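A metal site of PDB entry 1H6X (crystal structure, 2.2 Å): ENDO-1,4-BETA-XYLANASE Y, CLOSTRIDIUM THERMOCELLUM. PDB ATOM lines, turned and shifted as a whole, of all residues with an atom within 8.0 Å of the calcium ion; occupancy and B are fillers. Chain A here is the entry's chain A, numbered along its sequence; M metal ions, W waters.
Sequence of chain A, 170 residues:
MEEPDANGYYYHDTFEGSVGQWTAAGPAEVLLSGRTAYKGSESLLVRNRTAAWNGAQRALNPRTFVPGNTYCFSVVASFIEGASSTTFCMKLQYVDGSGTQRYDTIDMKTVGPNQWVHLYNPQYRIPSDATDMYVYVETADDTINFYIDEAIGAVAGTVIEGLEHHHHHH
The backbone carbonyl oxygen (O) of Glu 42 binds the calcium ion. Water W1 is bound to the calcium ion (2.3 Å). The calcium ion is bound by O of Thr 14 (2.3 Å). The calcium ion is bound by the backbone carbonyl oxygen (O) of Lys 39. OD1 of Asp 149 binds the calcium ion, at 2.5 Å. The calcium ion is bound by OE2 of Glu 16, 2.6 Å away. The side-chain carboxylate (OD2) of Asp 149 is bound to the calcium ion (2.7 Å).
Within 4 Å of the calcium ion: Thr 14, Glu 16, Lys 39, Glu 42 and Asp 149.
The backbone NH (N) of Gly 17 is in hydrogen-bond range of the side-chain carboxylate (OE1) of Glu 42, at 3.2 Å. The side-chain carboxylate (OD2) of Asp 149 lies close to the backbone NH (N) of Tyr 38, 2.9 Å away. The backbone NH (N) of Asp 149 is in hydrogen-bond range of the backbone carbonyl oxygen (O) of Val 76. The side-chain carboxylate (OE1) of Glu 16 lies within hydrogen-bond range of the side-chain hydroxyl (OG) of Ser 41 (2.8 Å).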
ATOM      1  N   HIS A  12     -28.078 -29.264 -23.299  1.00  0.00           N
ATOM      2  CA  HIS A  12     -26.985 -28.331 -23.517  1.00  0.00           C
ATOM      3  C   HIS A  12     -25.695 -29.064 -23.148  1.00  0.00           C
ATOM      4  O   HIS A  12     -25.382 -29.214 -21.977  1.00  0.00           O
ATOM      5  CB  HIS A  12     -27.167 -27.069 -22.670  1.00  0.00           C
ATOM      6  CG  HIS A  12     -26.065 -26.071 -22.846  1.00  0.00           C
ATOM      7  ND1 HIS A  12     -25.958 -24.933 -22.060  1.00  0.00           N
ATOM      8  CD2 HIS A  12     -25.029 -26.026 -23.712  1.00  0.00           C
ATOM      9  CE1 HIS A  12     -24.900 -24.240 -22.441  1.00  0.00           C
ATOM     10  NE2 HIS A  12     -24.323 -24.884 -23.443  1.00  0.00           N
ATOM     11  N   ASP A  13     -24.964 -29.510 -24.159  1.00  0.00           N
ATOM     12  CA  ASP A  13     -23.745 -30.272 -23.932  1.00  0.00           C
ATOM     13  C   ASP A  13     -22.482 -29.441 -24.145  1.00  0.00           C
ATOM     14  O   ASP A  13     -22.150 -29.083 -25.269  1.00  0.00           O
ATOM     15  CB  ASP A  13     -23.733 -31.498 -24.842  1.00  0.00           C
ATOM     16  CG  ASP A  13     -24.674 -32.573 -24.357  1.00  0.00           C
ATOM     17  OD1 ASP A  13     -24.400 -33.139 -23.279  1.00  0.00           O
ATOM     18  OD2 ASP A  13     -25.703 -32.922 -24.963  1.00  0.00           O
ATOM     19  N   THR A  14     -21.786 -29.130 -23.052  1.00  0.00           N
ATOM     20  CA  THR A  14     -20.534 -28.357 -23.104  1.00  0.00           C
ATOM     21  C   THR A  14     -19.339 -29.239 -23.309  1.00  0.00           C
ATOM     22  O   THR A  14     -18.275 -28.756 -23.683  1.00  0.00           O
ATOM     23  CB  THR A  14     -20.280 -27.633 -21.789  1.00  0.00           C
ATOM     24  OG1 THR A  14     -20.399 -28.576 -20.713  1.00  0.00           O
ATOM     25  CG2 THR A  14     -21.351 -26.569 -21.506  1.00  0.00           C
ATOM     26  N   PHE A  15     -19.497 -30.536 -23.029  1.00  0.00           N
ATOM     27  CA  PHE A  15     -18.406 -31.484 -23.169  1.00  0.00           C
ATOM     28  C   PHE A  15     -17.256 -31.134 -22.210  1.00  0.00           C
ATOM     29  O   PHE A  15     -16.071 -31.347 -22.499  1.00  0.00           O
ATOM     30  CB  PHE A  15     -17.952 -31.565 -24.627  1.00  0.00           C
ATOM     31  CG  PHE A  15     -19.046 -31.970 -25.583  1.00  0.00           C
ATOM     32  CD1 PHE A  15     -19.430 -31.130 -26.617  1.00  0.00           C
ATOM     33  CD2 PHE A  15     -19.691 -33.192 -25.442  1.00  0.00           C
ATOM     34  CE1 PHE A  15     -20.452 -31.511 -27.504  1.00  0.00           C
ATOM     35  CE2 PHE A  15     -20.719 -33.573 -26.321  1.00  0.00           C
ATOM     36  CZ  PHE A  15     -21.087 -32.731 -27.344  1.00  0.00           C
ATOM     37  N   GLU A  16     -17.631 -30.556 -21.076  1.00  0.00           N
ATOM     38  CA  GLU A  16     -16.661 -30.259 -20.031  1.00  0.00           C
ATOM     39  C   GLU A  16     -16.738 -31.363 -18.997  1.00  0.00           C
ATOM     40  O   GLU A  16     -17.485 -31.274 -18.016  1.00  0.00           O
ATOM     41  CB  GLU A  16     -16.942 -28.894 -19.392  1.00  0.00           C
ATOM     42  CG  GLU A  16     -16.911 -27.720 -20.374  1.00  0.00           C
ATOM     43  CD  GLU A  16     -15.551 -27.520 -21.019  1.00  0.00           C
ATOM     44  OE1 GLU A  16     -14.518 -27.720 -20.334  1.00  0.00           O
ATOM     45  OE2 GLU A  16     -15.501 -27.169 -22.207  1.00  0.00           O
ATOM     46  N   GLY A  17     -15.989 -32.438 -19.226  1.00  0.00           N
ATOM     47  CA  GLY A  17     -15.969 -33.549 -18.284  1.00  0.00           C
ATOM     48  C   GLY A  17     -16.956 -34.655 -18.593  1.00  0.00           C
ATOM     49  O   GLY A  17     -16.885 -35.729 -17.999  1.00  0.00           O
ATOM     50  N   LEU A  32     -13.963 -37.103 -25.234  1.00  0.00           N
ATOM     51  CA  LEU A  32     -13.669 -35.744 -24.830  1.00  0.00           C
ATOM     52  C   LEU A  32     -12.254 -35.405 -25.226  1.00  0.00           C
ATOM     53  O   LEU A  32     -11.381 -36.239 -25.151  1.00  0.00           O
ATOM     54  CB  LEU A  32     -13.841 -35.607 -23.321  1.00  0.00           C
ATOM     55  CG  LEU A  32     -15.238 -35.829 -22.760  1.00  0.00           C
ATOM     56  CD1 LEU A  32     -15.221 -35.770 -21.223  1.00  0.00           C
ATOM     57  CD2 LEU A  32     -16.221 -34.806 -23.326  1.00  0.00           C
ATOM     58  N   SER A  33     -12.011 -34.173 -25.676  1.00  0.00           N
ATOM     59  CA  SER A  33     -10.671 -33.760 -26.050  1.00  0.00           C
ATOM     60  C   SER A  33     -10.367 -32.305 -25.724  1.00  0.00           C
ATOM     61  O   SER A  33     -11.179 -31.417 -25.962  1.00  0.00           O
ATOM     62  CB  SER A  33     -10.406 -34.025 -27.521  1.00  0.00           C
ATOM     63  OG  SER A  33      -9.219 -33.372 -27.961  1.00  0.00           O
ATOM     64  N   THR A  36      -8.876 -28.751 -28.715  1.00  0.00           N
ATOM     65  CA  THR A  36      -9.490 -27.477 -29.079  1.00  0.00           C
ATOM     66  C   THR A  36     -10.860 -27.354 -28.408  1.00  0.00           C
ATOM     67  O   THR A  36     -11.467 -28.339 -28.017  1.00  0.00           O
ATOM     68  CB  THR A  36      -9.592 -27.324 -30.613  1.00  0.00           C
ATOM     69  OG1 THR A  36     -10.198 -26.067 -30.949  1.00  0.00           O
ATOM     70  CG2 THR A  36     -10.544 -28.337 -31.186  1.00  0.00           C
ATOM     71  N   ALA A  37     -11.343 -26.133 -28.257  1.00  0.00           N
ATOM     72  CA  ALA A  37     -12.617 -25.920 -27.608  1.00  0.00           C
ATOM     73  C   ALA A  37     -13.205 -24.625 -28.111  1.00  0.00           C
ATOM     74  O   ALA A  37     -12.503 -23.736 -28.570  1.00  0.00           O
ATOM     75  CB  ALA A  37     -12.430 -25.864 -26.092  1.00  0.00           C
ATOM     76  N   TYR A  38     -14.521 -24.525 -28.037  1.00  0.00           N
ATOM     77  CA  TYR A  38     -15.179 -23.325 -28.501  1.00  0.00           C
ATOM     78  C   TYR A  38     -15.482 -22.548 -27.250  1.00  0.00           C
ATOM     79  O   TYR A  38     -15.252 -21.344 -27.172  1.00  0.00           O
ATOM     80  CB  TYR A  38     -16.454 -23.692 -29.242  1.00  0.00           C
ATOM     81  CG  TYR A  38     -17.304 -22.502 -29.556  1.00  0.00           C
ATOM     82  CD1 TYR A  38     -16.891 -21.563 -30.490  1.00  0.00           C
ATOM     83  CD2 TYR A  38     -18.512 -22.311 -28.911  1.00  0.00           C
ATOM     84  CE1 TYR A  38     -17.669 -20.464 -30.780  1.00  0.00           C
ATOM     85  CE2 TYR A  38     -19.302 -21.223 -29.198  1.00  0.00           C
ATOM     86  CZ  TYR A  38     -18.879 -20.303 -30.124  1.00  0.00           C
ATOM     87  OH  TYR A  38     -19.666 -19.213 -30.397  1.00  0.00           O
ATOM     88  N   LYS A  39     -15.992 -23.260 -26.262  1.00  0.00           N
ATOM     89  CA  LYS A  39     -16.204 -22.730 -24.938  1.00  0.00           C
ATOM     90  C   LYS A  39     -15.621 -23.755 -23.977  1.00  0.00           C
ATOM     91  O   LYS A  39     -15.587 -24.958 -24.277  1.00  0.00           O
ATOM     92  CB  LYS A  39     -17.687 -22.480 -24.664  1.00  0.00           C
ATOM     93  CG  LYS A  39     -18.252 -21.251 -25.390  1.00  0.00           C
ATOM     94  CD  LYS A  39     -19.579 -20.774 -24.766  1.00  0.00           C
ATOM     95  CE  LYS A  39     -20.124 -19.556 -25.538  1.00  0.00           C
ATOM     96  NZ  LYS A  39     -21.504 -19.171 -25.104  1.00  0.00           N
ATOM     97  N   GLY A  40     -15.141 -23.283 -22.835  1.00  0.00           N
ATOM     98  CA  GLY A  40     -14.532 -24.172 -21.857  1.00  0.00           C
ATOM     99  C   GLY A  40     -13.181 -24.682 -22.286  1.00  0.00           C
ATOM    100  O   GLY A  40     -12.483 -24.053 -23.079  1.00  0.00           O
ATOM    101  N   SER A  41     -12.800 -25.849 -21.776  1.00  0.00           N
ATOM    102  CA  SER A  41     -11.496 -26.405 -22.104  1.00  0.00           C
ATOM    103  C   SER A  41     -11.607 -27.560 -23.083  1.00  0.00           C
ATOM    104  O   SER A  41     -10.600 -28.035 -23.604  1.00  0.00           O
ATOM    105  CB  SER A  41     -10.830 -26.879 -20.819  1.00  0.00           C
ATOM    106  OG  SER A  41     -11.717 -27.751 -20.135  1.00  0.00           O
ATOM    107  N   GLU A  42     -12.829 -28.031 -23.323  1.00  0.00           N
ATOM    108  CA  GLU A  42     -12.974 -29.208 -24.169  1.00  0.00           C
ATOM    109  C   GLU A  42     -14.142 -29.218 -25.131  1.00  0.00           C
ATOM    110  O   GLU A  42     -15.162 -28.530 -24.942  1.00  0.00           O
ATOM    111  CB  GLU A  42     -13.103 -30.453 -23.298  1.00  0.00           C
ATOM    112  CG  GLU A  42     -11.911 -30.771 -22.437  1.00  0.00           C
ATOM    113  CD  GLU A  42     -12.208 -31.897 -21.485  1.00  0.00           C
ATOM    114  OE1 GLU A  42     -13.328 -31.958 -20.949  1.00  0.00           O
ATOM    115  OE2 GLU A  42     -11.310 -32.739 -21.299  1.00  0.00           O
ATOM    116  N   SER A  43     -13.994 -30.054 -26.148  1.00  0.00           N
ATOM    117  CA  SER A  43     -15.032 -30.302 -27.118  1.00  0.00           C
ATOM    118  C   SER A  43     -15.089 -31.816 -27.271  1.00  0.00           C
ATOM    119  O   SER A  43     -14.308 -32.543 -26.637  1.00  0.00           O
ATOM    120  CB  SER A  43     -14.663 -29.654 -28.447  1.00  0.00           C
ATOM    121  OG  SER A  43     -13.453 -30.194 -28.931  1.00  0.00           O
ATOM    122  N   LEU A  44     -16.005 -32.292 -28.112  1.00  0.00           N
ATOM    123  CA  LEU A  44     -16.125 -33.711 -28.379  1.00  0.00           C
ATOM    124  C   LEU A  44     -15.398 -34.021 -29.680  1.00  0.00           C
ATOM    125  O   LEU A  44     -15.652 -33.398 -30.710  1.00  0.00           O
ATOM    126  CB  LEU A  44     -17.588 -34.147 -28.478  1.00  0.00           C
ATOM    127  CG  LEU A  44     -17.780 -35.660 -28.684  1.00  0.00           C
ATOM    128  CD1 LEU A  44     -17.587 -36.417 -27.358  1.00  0.00           C
ATOM    129  CD2 LEU A  44     -19.146 -35.934 -29.271  1.00  0.00           C
ATOM    130  N   VAL A  76     -21.648 -26.322 -32.675  1.00  0.00           N
ATOM    131  CA  VAL A  76     -20.559 -25.681 -33.369  1.00  0.00           C
ATOM    132  C   VAL A  76     -19.559 -26.766 -33.686  1.00  0.00           C
ATOM    133  O   VAL A  76     -19.365 -27.709 -32.907  1.00  0.00           O
ATOM    134  CB  VAL A  76     -19.935 -24.524 -32.569  1.00  0.00           C
ATOM    135  CG1 VAL A  76     -20.981 -23.441 -32.330  1.00  0.00           C
ATOM    136  CG2 VAL A  76     -19.382 -25.028 -31.251  1.00  0.00           C
ATOM    137  N   TRP A 116     -14.234 -22.416 -36.077  1.00  0.00           N
ATOM    138  CA  TRP A 116     -15.546 -22.873 -35.661  1.00  0.00           C
ATOM    139  C   TRP A 116     -16.604 -22.366 -36.628  1.00  0.00           C
ATOM    140  O   TRP A 116     -16.503 -21.247 -37.147  1.00  0.00           O
ATOM    141  CB  TRP A 116     -15.829 -22.471 -34.215  1.00  0.00           C
ATOM    142  CG  TRP A 116     -14.912 -23.186 -33.254  1.00  0.00           C
ATOM    143  CD1 TRP A 116     -13.772 -22.686 -32.673  1.00  0.00           C
ATOM    144  CD2 TRP A 116     -15.024 -24.543 -32.788  1.00  0.00           C
ATOM    145  NE1 TRP A 116     -13.195 -23.635 -31.871  1.00  0.00           N
ATOM    146  CE2 TRP A 116     -13.928 -24.783 -31.930  1.00  0.00           C
ATOM    147  CE3 TRP A 116     -15.943 -25.575 -33.018  1.00  0.00           C
ATOM    148  CZ2 TRP A 116     -13.744 -26.011 -31.286  1.00  0.00           C
ATOM    149  CZ3 TRP A 116     -15.749 -26.793 -32.390  1.00  0.00           C
ATOM    150  CH2 TRP A 116     -14.662 -27.003 -31.526  1.00  0.00           C
ATOM    151  N   ILE A 148     -16.873 -31.131 -32.028  1.00  0.00           N
ATOM    152  CA  ILE A 148     -18.112 -30.396 -31.827  1.00  0.00           C
ATOM    153  C   ILE A 148     -18.185 -29.931 -30.388  1.00  0.00           C
ATOM    154  O   ILE A 148     -17.576 -30.524 -29.485  1.00  0.00           O
ATOM    155  CB  ILE A 148     -19.377 -31.207 -32.211  1.00  0.00           C
ATOM    156  CG1 ILE A 148     -19.666 -32.284 -31.172  1.00  0.00           C
ATOM    157  CG2 ILE A 148     -19.259 -31.775 -33.620  1.00  0.00           C
ATOM    158  CD1 ILE A 148     -20.903 -33.125 -31.479  1.00  0.00           C
ATOM    159  N   ASP A 149     -18.962 -28.879 -30.164  1.00  0.00           N
ATOM    160  CA  ASP A 149     -19.040 -28.284 -28.861  1.00  0.00           C
ATOM    161  C   ASP A 149     -20.371 -27.570 -28.791  1.00  0.00           C
ATOM    162  O   ASP A 149     -21.010 -27.334 -29.817  1.00  0.00           O
ATOM    163  CB  ASP A 149     -17.879 -27.282 -28.701  1.00  0.00           C
ATOM    164  CG  ASP A 149     -17.552 -26.942 -27.251  1.00  0.00           C
ATOM    165  OD1 ASP A 149     -18.324 -27.336 -26.330  1.00  0.00           O
ATOM    166  OD2 ASP A 149     -16.535 -26.276 -26.931  1.00  0.00           O
ATOM    167  N   GLU A 150     -20.811 -27.276 -27.577  1.00  0.00           N
ATOM    168  CA  GLU A 150     -22.046 -26.531 -27.385  1.00  0.00           C
ATOM    169  C   GLU A 150     -23.238 -27.055 -28.179  1.00  0.00           C
ATOM    170  O   GLU A 150     -23.954 -26.281 -28.831  1.00  0.00           O
ATOM    171  CB  GLU A 150     -21.787 -25.046 -27.721  1.00  0.00           C
ATOM    172  CG  GLU A 150     -21.045 -24.305 -26.626  1.00  0.00           C
ATOM    173  CD  GLU A 150     -21.856 -24.219 -25.341  1.00  0.00           C
ATOM    174  OE1 GLU A 150     -21.328 -24.617 -24.290  1.00  0.00           O
ATOM    175  OE2 GLU A 150     -23.015 -23.768 -25.395  1.00  0.00           O
ATOM    176  N   ALA A 151     -23.467 -28.370 -28.136  1.00  0.00           N
ATOM    177  CA  ALA A 151     -24.637 -28.940 -28.783  1.00  0.00           C
ATOM    178  C   ALA A 151     -25.872 -28.625 -27.943  1.00  0.00           C
ATOM    179  O   ALA A 151     -25.933 -28.948 -26.763  1.00  0.00           O
ATOM    180  CB  ALA A 151     -24.485 -30.435 -29.003  1.00  0.00           C
HETATM  181 CA    CA M   1     -16.815 -27.085 -24.397  1.00  0.00          CA
HETATM  182  O   HOH W   1     -18.478 -25.647 -23.668  1.00  0.00           O
